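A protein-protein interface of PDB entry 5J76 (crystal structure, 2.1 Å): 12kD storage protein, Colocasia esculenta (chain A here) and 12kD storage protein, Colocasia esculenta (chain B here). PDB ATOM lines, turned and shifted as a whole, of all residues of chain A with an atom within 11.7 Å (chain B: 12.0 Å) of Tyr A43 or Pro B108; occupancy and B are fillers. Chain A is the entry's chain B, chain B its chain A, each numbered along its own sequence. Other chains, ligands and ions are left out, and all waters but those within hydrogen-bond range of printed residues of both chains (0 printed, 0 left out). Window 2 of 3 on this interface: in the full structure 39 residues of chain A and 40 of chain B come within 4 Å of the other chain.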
ATOM      1  N   ASN A  25      16.717  -2.618  -4.743  1.00  0.00           N
ATOM      2  CA  ASN A  25      16.053  -2.782  -3.426  1.00  0.00           C
ATOM      3  C   ASN A  25      15.024  -1.732  -3.026  1.00  0.00           C
ATOM      4  O   ASN A  25      14.585  -1.765  -1.872  1.00  0.00           O
ATOM      5  CB  ASN A  25      17.043  -2.845  -2.220  1.00  0.00           C
ATOM      6  CG  ASN A  25      18.116  -3.886  -2.386  1.00  0.00           C
ATOM      7  OD1 ASN A  25      19.297  -3.596  -2.309  1.00  0.00           O
ATOM      8  ND2 ASN A  25      17.712  -5.041  -2.737  1.00  0.00           N
ATOM      9  N   HIS A  26      14.644  -0.819  -3.918  1.00  0.00           N
ATOM     10  CA  HIS A  26      13.715   0.270  -3.540  1.00  0.00           C
ATOM     11  C   HIS A  26      12.746   0.606  -4.630  1.00  0.00           C
ATOM     12  O   HIS A  26      13.051   0.428  -5.786  1.00  0.00           O
ATOM     13  CB  HIS A  26      14.475   1.525  -3.171  1.00  0.00           C
ATOM     14  CG  HIS A  26      15.262   1.377  -1.929  1.00  0.00           C
ATOM     15  ND1 HIS A  26      16.542   0.871  -1.926  1.00  0.00           N
ATOM     16  CD2 HIS A  26      14.935   1.606  -0.631  1.00  0.00           C
ATOM     17  CE1 HIS A  26      16.990   0.837  -0.678  1.00  0.00           C
ATOM     18  NE2 HIS A  26      16.035   1.283   0.124  1.00  0.00           N
ATOM     19  N   GLN A  27      11.582   1.125  -4.243  1.00  0.00           N
ATOM     20  CA  GLN A  27      10.578   1.603  -5.186  1.00  0.00           C
ATOM     21  C   GLN A  27       9.976   2.828  -4.605  1.00  0.00           C
ATOM     22  O   GLN A  27       9.827   2.912  -3.408  1.00  0.00           O
ATOM     23  CB  GLN A  27       9.504   0.567  -5.390  1.00  0.00           C
ATOM     24  CG  GLN A  27      10.061  -0.615  -6.127  1.00  0.00           C
ATOM     25  CD  GLN A  27       9.010  -1.647  -6.490  1.00  0.00           C
ATOM     26  OE1 GLN A  27       7.864  -1.403  -6.418  1.00  0.00           O
ATOM     27  NE2 GLN A  27       9.451  -2.818  -6.854  1.00  0.00           N
ATOM     28  N   LEU A  28       9.724   3.827  -5.442  1.00  0.00           N
ATOM     29  CA  LEU A  28       9.034   5.091  -4.986  1.00  0.00           C
ATOM     30  C   LEU A  28       7.721   5.106  -5.798  1.00  0.00           C
ATOM     31  O   LEU A  28       7.796   5.313  -7.013  1.00  0.00           O
ATOM     32  CB  LEU A  28       9.892   6.292  -5.297  1.00  0.00           C
ATOM     33  CG  LEU A  28       9.247   7.643  -4.939  1.00  0.00           C
ATOM     34  CD1 LEU A  28       8.914   7.689  -3.420  1.00  0.00           C
ATOM     35  CD2 LEU A  28      10.171   8.773  -5.412  1.00  0.00           C
ATOM     36  N   ASN A  35      -1.240   8.259  -1.717  1.00  0.00           N
ATOM     37  CA  ASN A  35      -0.040   8.288  -0.840  1.00  0.00           C
ATOM     38  C   ASN A  35       1.186   7.976  -1.673  1.00  0.00           C
ATOM     39  O   ASN A  35       1.144   7.023  -2.463  1.00  0.00           O
ATOM     40  CB  ASN A  35      -0.172   7.174   0.204  1.00  0.00           C
ATOM     41  CG  ASN A  35       0.674   7.398   1.438  1.00  0.00           C
ATOM     42  OD1 ASN A  35       1.123   8.510   1.763  1.00  0.00           O
ATOM     43  ND2 ASN A  35       0.810   6.347   2.175  1.00  0.00           N
ATOM     44  N   LEU A  36       2.249   8.744  -1.471  1.00  0.00           N
ATOM     45  CA  LEU A  36       3.556   8.517  -2.142  1.00  0.00           C
ATOM     46  C   LEU A  36       4.409   7.779  -1.127  1.00  0.00           C
ATOM     47  O   LEU A  36       4.661   8.303  -0.040  1.00  0.00           O
ATOM     48  CB  LEU A  36       4.195   9.867  -2.527  1.00  0.00           C
ATOM     49  CG  LEU A  36       5.589   9.819  -3.159  1.00  0.00           C
ATOM     50  CD1 LEU A  36       5.511   9.114  -4.505  1.00  0.00           C
ATOM     51  CD2 LEU A  36       6.160  11.201  -3.312  1.00  0.00           C
ATOM     52  N   VAL A  37       4.865   6.595  -1.483  1.00  0.00           N
ATOM     53  CA  VAL A  37       5.563   5.724  -0.577  1.00  0.00           C
ATOM     54  C   VAL A  37       6.869   5.226  -1.215  1.00  0.00           C
ATOM     55  O   VAL A  37       6.904   4.651  -2.345  1.00  0.00           O
ATOM     56  CB  VAL A  37       4.704   4.474  -0.194  1.00  0.00           C
ATOM     57  CG1 VAL A  37       5.429   3.566   0.837  1.00  0.00           C
ATOM     58  CG2 VAL A  37       3.300   4.893   0.259  1.00  0.00           C
ATOM     59  N   LEU A  38       7.916   5.300  -0.404  1.00  0.00           N
ATOM     60  CA  LEU A  38       9.224   4.715  -0.699  1.00  0.00           C
ATOM     61  C   LEU A  38       9.327   3.376   0.016  1.00  0.00           C
ATOM     62  O   LEU A  38       9.381   3.302   1.220  1.00  0.00           O
ATOM     63  CB  LEU A  38      10.355   5.684  -0.272  1.00  0.00           C
ATOM     64  CG  LEU A  38      11.699   5.396  -0.989  1.00  0.00           C
ATOM     65  CD1 LEU A  38      12.694   6.477  -0.663  1.00  0.00           C
ATOM     66  CD2 LEU A  38      12.305   4.073  -0.632  1.00  0.00           C
ATOM     67  N   TYR A  39       9.326   2.323  -0.764  1.00  0.00           N
ATOM     68  CA  TYR A  39       9.419   0.967  -0.316  1.00  0.00           C
ATOM     69  C   TYR A  39      10.861   0.490  -0.288  1.00  0.00           C
ATOM     70  O   TYR A  39      11.597   0.705  -1.231  1.00  0.00           O
ATOM     71  CB  TYR A  39       8.642   0.024  -1.252  1.00  0.00           C
ATOM     72  CG  TYR A  39       7.176   0.154  -1.000  1.00  0.00           C
ATOM     73  CD1 TYR A  39       6.591  -0.449   0.109  1.00  0.00           C
ATOM     74  CD2 TYR A  39       6.357   0.937  -1.840  1.00  0.00           C
ATOM     75  CE1 TYR A  39       5.226  -0.297   0.404  1.00  0.00           C
ATOM     76  CE2 TYR A  39       4.976   1.101  -1.569  1.00  0.00           C
ATOM     77  CZ  TYR A  39       4.414   0.485  -0.450  1.00  0.00           C
ATOM     78  OH  TYR A  39       3.078   0.646  -0.195  1.00  0.00           O
ATOM     79  N   GLY A  40      11.228  -0.212   0.801  1.00  0.00           N
ATOM     80  CA  GLY A  40      12.473  -0.947   0.892  1.00  0.00           C
ATOM     81  C   GLY A  40      13.199  -0.452   2.100  1.00  0.00           C
ATOM     82  O   GLY A  40      12.694   0.361   2.846  1.00  0.00           O
ATOM     83  N   GLY A  41      14.436  -0.914   2.254  1.00  0.00           N
ATOM     84  CA  GLY A  41      15.065  -0.799   3.552  1.00  0.00           C
ATOM     85  C   GLY A  41      15.527   0.598   3.794  1.00  0.00           C
ATOM     86  O   GLY A  41      15.754   1.297   2.819  1.00  0.00           O
ATOM     87  N   LYS A  42      15.698   1.022   5.052  1.00  0.00           N
ATOM     88  CA  LYS A  42      15.351   0.303   6.301  1.00  0.00           C
ATOM     89  C   LYS A  42      13.914   0.513   6.629  1.00  0.00           C
ATOM     90  O   LYS A  42      13.112  -0.367   6.498  1.00  0.00           O
ATOM     91  CB  LYS A  42      16.136   0.835   7.515  1.00  0.00           C
ATOM     92  CG  LYS A  42      17.202  -0.101   7.949  1.00  0.00           C
ATOM     93  CD  LYS A  42      18.050   0.492   9.028  1.00  0.00           C
ATOM     94  CE  LYS A  42      19.402  -0.206   8.963  1.00  0.00           C
ATOM     95  NZ  LYS A  42      20.157   0.274  10.123  1.00  0.00           N
ATOM     96  N   TYR A  43      13.639   1.726   7.068  1.00  0.00           N
ATOM     97  CA  TYR A  43      12.315   2.205   7.434  1.00  0.00           C
ATOM     98  C   TYR A  43      11.341   2.473   6.249  1.00  0.00           C
ATOM     99  O   TYR A  43      10.119   2.428   6.395  1.00  0.00           O
ATOM    100  CB  TYR A  43      12.490   3.586   7.959  1.00  0.00           C
ATOM    101  CG  TYR A  43      12.997   3.759   9.332  1.00  0.00           C
ATOM    102  CD1 TYR A  43      12.072   4.028  10.341  1.00  0.00           C
ATOM    103  CD2 TYR A  43      14.384   3.703   9.656  1.00  0.00           C
ATOM    104  CE1 TYR A  43      12.476   4.226  11.646  1.00  0.00           C
ATOM    105  CE2 TYR A  43      14.806   3.922  10.960  1.00  0.00           C
ATOM    106  CZ  TYR A  43      13.827   4.184  11.942  1.00  0.00           C
ATOM    107  OH  TYR A  43      14.117   4.457  13.257  1.00  0.00           O
ATOM    108  N   GLY A  44      11.848   2.960   5.129  1.00  0.00           N
ATOM    109  CA  GLY A  44      10.928   3.462   4.089  1.00  0.00           C
ATOM    110  C   GLY A  44      10.456   4.859   4.463  1.00  0.00           C
ATOM    111  O   GLY A  44      10.974   5.463   5.389  1.00  0.00           O
ATOM    112  N   TRP A  45       9.450   5.345   3.756  1.00  0.00           N
ATOM    113  CA  TRP A  45       8.937   6.690   3.924  1.00  0.00           C
ATOM    114  C   TRP A  45       7.582   6.779   3.245  1.00  0.00           C
ATOM    115  O   TRP A  45       7.315   6.042   2.249  1.00  0.00           O
ATOM    116  CB  TRP A  45       9.912   7.660   3.239  1.00  0.00           C
ATOM    117  CG  TRP A  45       9.523   9.128   3.233  1.00  0.00           C
ATOM    118  CD1 TRP A  45       9.887  10.038   4.139  1.00  0.00           C
ATOM    119  CD2 TRP A  45       8.748   9.837   2.242  1.00  0.00           C
ATOM    120  NE1 TRP A  45       9.365  11.264   3.808  1.00  0.00           N
ATOM    121  CE2 TRP A  45       8.668  11.163   2.641  1.00  0.00           C
ATOM    122  CE3 TRP A  45       8.122   9.472   1.064  1.00  0.00           C
ATOM    123  CZ2 TRP A  45       7.949  12.121   1.929  1.00  0.00           C
ATOM    124  CZ3 TRP A  45       7.402  10.447   0.350  1.00  0.00           C
ATOM    125  CH2 TRP A  45       7.342  11.733   0.765  1.00  0.00           C
ATOM    126  N   GLN A  46       6.781   7.743   3.709  1.00  0.00           N
ATOM    127  CA  GLN A  46       5.586   8.097   3.003  1.00  0.00           C
ATOM    128  C   GLN A  46       5.274   9.522   3.130  1.00  0.00           C
ATOM    129  O   GLN A  46       5.652  10.163   4.086  1.00  0.00           O
ATOM    130  CB  GLN A  46       4.414   7.268   3.519  1.00  0.00           C
ATOM    131  CG  GLN A  46       4.132   7.540   4.983  1.00  0.00           C
ATOM    132  CD  GLN A  46       3.098   6.608   5.498  1.00  0.00           C
ATOM    133  OE1 GLN A  46       2.011   6.525   4.948  1.00  0.00           O
ATOM    134  NE2 GLN A  46       3.446   5.849   6.492  1.00  0.00           N
ATOM    135  N   SER A  47       4.511  10.020   2.176  1.00  0.00           N
ATOM    136  CA  SER A  47       4.006  11.387   2.224  1.00  0.00           C
ATOM    137  C   SER A  47       2.892  11.503   3.253  1.00  0.00           C
ATOM    138  O   SER A  47       2.532  12.599   3.639  1.00  0.00           O
ATOM    139  CB  SER A  47       3.430  11.823   0.858  1.00  0.00           C
ATOM    140  OG  SER A  47       2.384  10.953   0.445  1.00  0.00           O
ATOM    141  N   ASN A  48       2.269  10.379   3.565  1.00  0.00           N
ATOM    142  CA  ASN A  48       1.255  10.278   4.576  1.00  0.00           C
ATOM    143  C   ASN A  48      -0.032  10.929   4.073  1.00  0.00           C
ATOM    144  O   ASN A  48      -0.572  11.841   4.717  1.00  0.00           O
ATOM    145  CB  ASN A  48       1.741  10.945   5.911  1.00  0.00           C
ATOM    146  CG  ASN A  48       0.898  10.508   7.099  1.00  0.00           C
ATOM    147  OD1 ASN A  48       0.378   9.419   7.119  1.00  0.00           O
ATOM    148  ND2 ASN A  48       0.765  11.366   8.086  1.00  0.00           N
ATOM    149  N   ASP A  95      21.540   3.569  -3.667  1.00  0.00           N
ATOM    150  CA  ASP A  95      21.565   3.518  -2.200  1.00  0.00           C
ATOM    151  C   ASP A  95      20.229   3.826  -1.493  1.00  0.00           C
ATOM    152  O   ASP A  95      20.245   3.976  -0.309  1.00  0.00           O
ATOM    153  CB  ASP A  95      22.684   4.435  -1.677  1.00  0.00           C
ATOM    154  CG  ASP A  95      22.408   5.865  -1.950  1.00  0.00           C
ATOM    155  OD1 ASP A  95      21.335   6.245  -2.481  1.00  0.00           O
ATOM    156  OD2 ASP A  95      23.261   6.668  -1.599  1.00  0.00           O
ATOM    157  N   GLY A  96      19.080   3.948  -2.178  1.00  0.00           N
ATOM    158  CA  GLY A  96      17.800   4.127  -1.467  1.00  0.00           C
ATOM    159  C   GLY A  96      17.307   5.550  -1.279  1.00  0.00           C
ATOM    160  O   GLY A  96      16.083   5.780  -1.087  1.00  0.00           O
ATOM    161  N   PHE A  97      18.220   6.516  -1.375  1.00  0.00           N
ATOM    162  CA  PHE A  97      17.867   7.935  -1.280  1.00  0.00           C
ATOM    163  C   PHE A  97      17.199   8.368  -2.604  1.00  0.00           C
ATOM    164  O   PHE A  97      17.618   7.898  -3.664  1.00  0.00           O
ATOM    165  CB  PHE A  97      19.128   8.773  -1.094  1.00  0.00           C
ATOM    166  CG  PHE A  97      19.667   8.780   0.321  1.00  0.00           C
ATOM    167  CD1 PHE A  97      19.239   9.726   1.243  1.00  0.00           C
ATOM    168  CD2 PHE A  97      20.628   7.849   0.727  1.00  0.00           C
ATOM    169  CE1 PHE A  97      19.754   9.739   2.560  1.00  0.00           C
ATOM    170  CE2 PHE A  97      21.164   7.864   2.045  1.00  0.00           C
ATOM    171  CZ  PHE A  97      20.715   8.799   2.963  1.00  0.00           C
ATOM    172  N   LYS B 102      15.727  15.680  -0.534  1.00  0.00           N
ATOM    173  CA  LYS B 102      16.190  14.318  -0.310  1.00  0.00           C
ATOM    174  C   LYS B 102      15.085  13.567   0.454  1.00  0.00           C
ATOM    175  O   LYS B 102      14.438  14.162   1.289  1.00  0.00           O
ATOM    176  CB  LYS B 102      17.435  14.427   0.523  1.00  0.00           C
ATOM    177  CG  LYS B 102      18.357  13.263   0.459  1.00  0.00           C
ATOM    178  CD  LYS B 102      19.623  13.558   1.260  1.00  0.00           C
ATOM    179  CE  LYS B 102      19.342  13.430   2.750  1.00  0.00           C
ATOM    180  NZ  LYS B 102      19.663  14.662   3.493  1.00  0.00           N
ATOM    181  N   ILE B 103      14.770  12.337   0.087  1.00  0.00           N
ATOM    182  CA  ILE B 103      13.949  11.475   0.891  1.00  0.00           C
ATOM    183  C   ILE B 103      14.883  10.380   1.360  1.00  0.00           C
ATOM    184  O   ILE B 103      15.574   9.725   0.573  1.00  0.00           O
ATOM    185  CB  ILE B 103      12.799  10.884   0.126  1.00  0.00           C
ATOM    186  CG1 ILE B 103      11.797  11.963  -0.244  1.00  0.00           C
ATOM    187  CG2 ILE B 103      12.063   9.856   0.952  1.00  0.00           C
ATOM    188  CD1 ILE B 103      10.822  11.446  -1.267  1.00  0.00           C
ATOM    189  N   ASP B 104      14.921  10.177   2.652  1.00  0.00           N
ATOM    190  CA  ASP B 104      15.830   9.244   3.291  1.00  0.00           C
ATOM    191  C   ASP B 104      15.059   8.103   3.998  1.00  0.00           C
ATOM    192  O   ASP B 104      14.506   8.313   5.071  1.00  0.00           O
ATOM    193  CB  ASP B 104      16.632   9.983   4.327  1.00  0.00           C
ATOM    194  CG  ASP B 104      17.695   9.100   4.937  1.00  0.00           C
ATOM    195  OD1 ASP B 104      17.581   7.858   4.805  1.00  0.00           O
ATOM    196  OD2 ASP B 104      18.675   9.647   5.475  1.00  0.00           O
ATOM    197  N   PRO B 105      15.047   6.889   3.415  1.00  0.00           N
ATOM    198  CA  PRO B 105      14.358   5.769   4.019  1.00  0.00           C
ATOM    199  C   PRO B 105      15.185   5.000   5.096  1.00  0.00           C
ATOM    200  O   PRO B 105      14.747   3.945   5.565  1.00  0.00           O
ATOM    201  CB  PRO B 105      14.139   4.851   2.835  1.00  0.00           C
ATOM    202  CG  PRO B 105      15.438   4.995   2.090  1.00  0.00           C
ATOM    203  CD  PRO B 105      15.852   6.436   2.258  1.00  0.00           C
ATOM    204  N   TRP B 106      16.366   5.484   5.436  1.00  0.00           N
ATOM    205  CA  TRP B 106      17.197   4.805   6.409  1.00  0.00           C
ATOM    206  C   TRP B 106      16.918   5.217   7.868  1.00  0.00           C
ATOM    207  O   TRP B 106      17.383   4.540   8.776  1.00  0.00           O
ATOM    208  CB  TRP B 106      18.661   5.027   6.053  1.00  0.00           C
ATOM    209  CG  TRP B 106      18.959   4.503   4.688  1.00  0.00           C
ATOM    210  CD1 TRP B 106      19.121   5.234   3.545  1.00  0.00           C
ATOM    211  CD2 TRP B 106      19.050   3.124   4.290  1.00  0.00           C
ATOM    212  NE1 TRP B 106      19.343   4.402   2.478  1.00  0.00           N
ATOM    213  CE2 TRP B 106      19.317   3.103   2.911  1.00  0.00           C
ATOM    214  CE3 TRP B 106      18.955   1.905   4.970  1.00  0.00           C
ATOM    215  CZ2 TRP B 106      19.466   1.903   2.193  1.00  0.00           C
ATOM    216  CZ3 TRP B 106      19.118   0.721   4.253  1.00  0.00           C
ATOM    217  CH2 TRP B 106      19.363   0.734   2.884  1.00  0.00           C
ATOM    218  N   VAL B 107      16.141   6.282   8.085  1.00  0.00           N
ATOM    219  CA  VAL B 107      15.941   6.875   9.412  1.00  0.00           C
ATOM    220  C   VAL B 107      14.455   7.066   9.580  1.00  0.00           C
ATOM    221  O   VAL B 107      13.770   7.144   8.590  1.00  0.00           O
ATOM    222  CB  VAL B 107      16.697   8.229   9.570  1.00  0.00           C
ATOM    223  CG1 VAL B 107      18.164   8.053   9.243  1.00  0.00           C
ATOM    224  CG2 VAL B 107      16.085   9.338   8.718  1.00  0.00           C
ATOM    225  N   PRO B 108      13.948   7.159  10.834  1.00  0.00           N
ATOM    226  CA  PRO B 108      12.480   7.377  11.096  1.00  0.00           C
ATOM    227  C   PRO B 108      11.938   8.756  10.643  1.00  0.00           C
ATOM    228  O   PRO B 108      12.755   9.636  10.329  1.00  0.00           O
ATOM    229  CB  PRO B 108      12.381   7.284  12.644  1.00  0.00           C
ATOM    230  CG  PRO B 108      13.759   7.559  13.168  1.00  0.00           C
ATOM    231  CD  PRO B 108      14.765   7.286  12.070  1.00  0.00           C
ATOM    232  N   GLY B 109      10.613   8.992  10.658  1.00  0.00           N
ATOM    233  CA  GLY B 109       9.570   8.039  11.092  1.00  0.00           C
ATOM    234  C   GLY B 109       9.145   7.131   9.955  1.00  0.00           C
ATOM    235  O   GLY B 109       9.157   5.909  10.104  1.00  0.00           O
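O of Pro B105 sits at hydrogen-bond distance from N of Lys A42 (3.1 Å).
The indole nitrogen (NE1) of Trp B106 is in hydrogen-bond range of the backbone carbonyl oxygen (O) of Asp A95 (3.0 Å).
The backbone carbonyl oxygen (O) of Pro B105 is in hydrogen-bond range of the backbone NH (N) of Tyr A43 (2.9 Å).
O of Pro B105 lies within hydrogen-bond range of N of Gly A44 (3.1 Å).
OD1 of Asp B104 sits at hydrogen-bond distance from N of Trp B106 (2.7 Å).
N of Leu A38 sits at hydrogen-bond distance from O of Trp A45, 2.8 Å away.
The backbone carbonyl oxygen (O) of Gly A41 is in hydrogen-bond range of a ring nitrogen (NE2) of His A26 (2.7 Å).
The side-chain carboxylate (OD1) of Asp A95 sits at hydrogen-bond distance from the backbone NH (N) of Phe A97 (3.3 Å).
Among the printed residues, pairs that only touch across the chains: Phe A97 with Asp B104, Tyr A43 with Pro B108, Tyr A43 with Trp B106, Gly A96 with Pro B105, Tyr A43 with Val B107, Lys A42 with Trp B106, Phe A97 with Ile B103, Tyr A43 with Gly B109, Trp A45 with Ile B103, Gly A41 with Trp B106, Phe A97 with Trp B106, Phe A97 with Lys B102, Gly A41 with Pro B105, Leu A38 with Ile B103, His A26 with Trp B106 and Leu A38 with Pro B105.
Tyr A43 touches just these residues of chain B: Pro B105 (2.9 Å), Trp B106 (3.2 Å), Val B107 (3.4 Å), Pro B108 (3.1 Å) and Gly B109 (3.5 Å).
Pro B108 touches just one residue of chain A: Tyr A43 (3.1 Å).
Gly A40 touches none of the printed residues of chain B.
Of chain B, only Pro B105 and Trp B106 come within 4 Å of Gly A41.
Of chain B, only Pro B105 (3.1 Å) and Trp B106 (3.4 Å) come within 4 Å of Lys A42.
Gly A44 touches just one residue of chain B: Pro B105 (3.1 Å).
Val B107 touches one residue of chain A.
Of chain A, only Tyr A43 (3.5 Å) comes within 4 Å of Gly B109.
Of the printed residues of chain B, Trp A45 touches Ile B103 (3.5 Å).
Printed residues of chain B within 4 Å of Leu A38: Ile B103 and Pro B105.
Of the printed residues of chain B, Phe A97 touches Lys B102 (3.7 Å), Ile B103 (3.4 Å), Asp B104 (3.1 Å) and Trp B106 (3.7 Å).
Of the printed residues of chain A, Trp B106 touches His A26, Gly A41, Lys A42, Tyr A43, Asp A95 and Phe A97.
Asn A25 touches none of the printed residues of chain B.
The nearest residue of chain B that does not touch Tyr A43 is Asp B104 (5.9 Å).
The nearest residue of chain A that does not touch Pro B108 is Gly A44 (6.2 Å).
Hydrophobic or aromatic side chains of chain B that line the printed part of chain A: Ile B103, Pro B105, Trp B106 and Pro B108.
Hydrophobic or aromatic side chains of chain A that line the printed part of chain B: His A26, Leu A38, Tyr A43, Trp A45 and Phe A97.
Along chain A the printed residues that touch a printed residue of chain B span positions 26 to 97.
Among the printed residues, 20 pairs touch across the chains.
Among the printed residues, no Asp or Glu carboxylate lies within 4 Å of a Lys or Arg side-chain nitrogen of the other chain.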
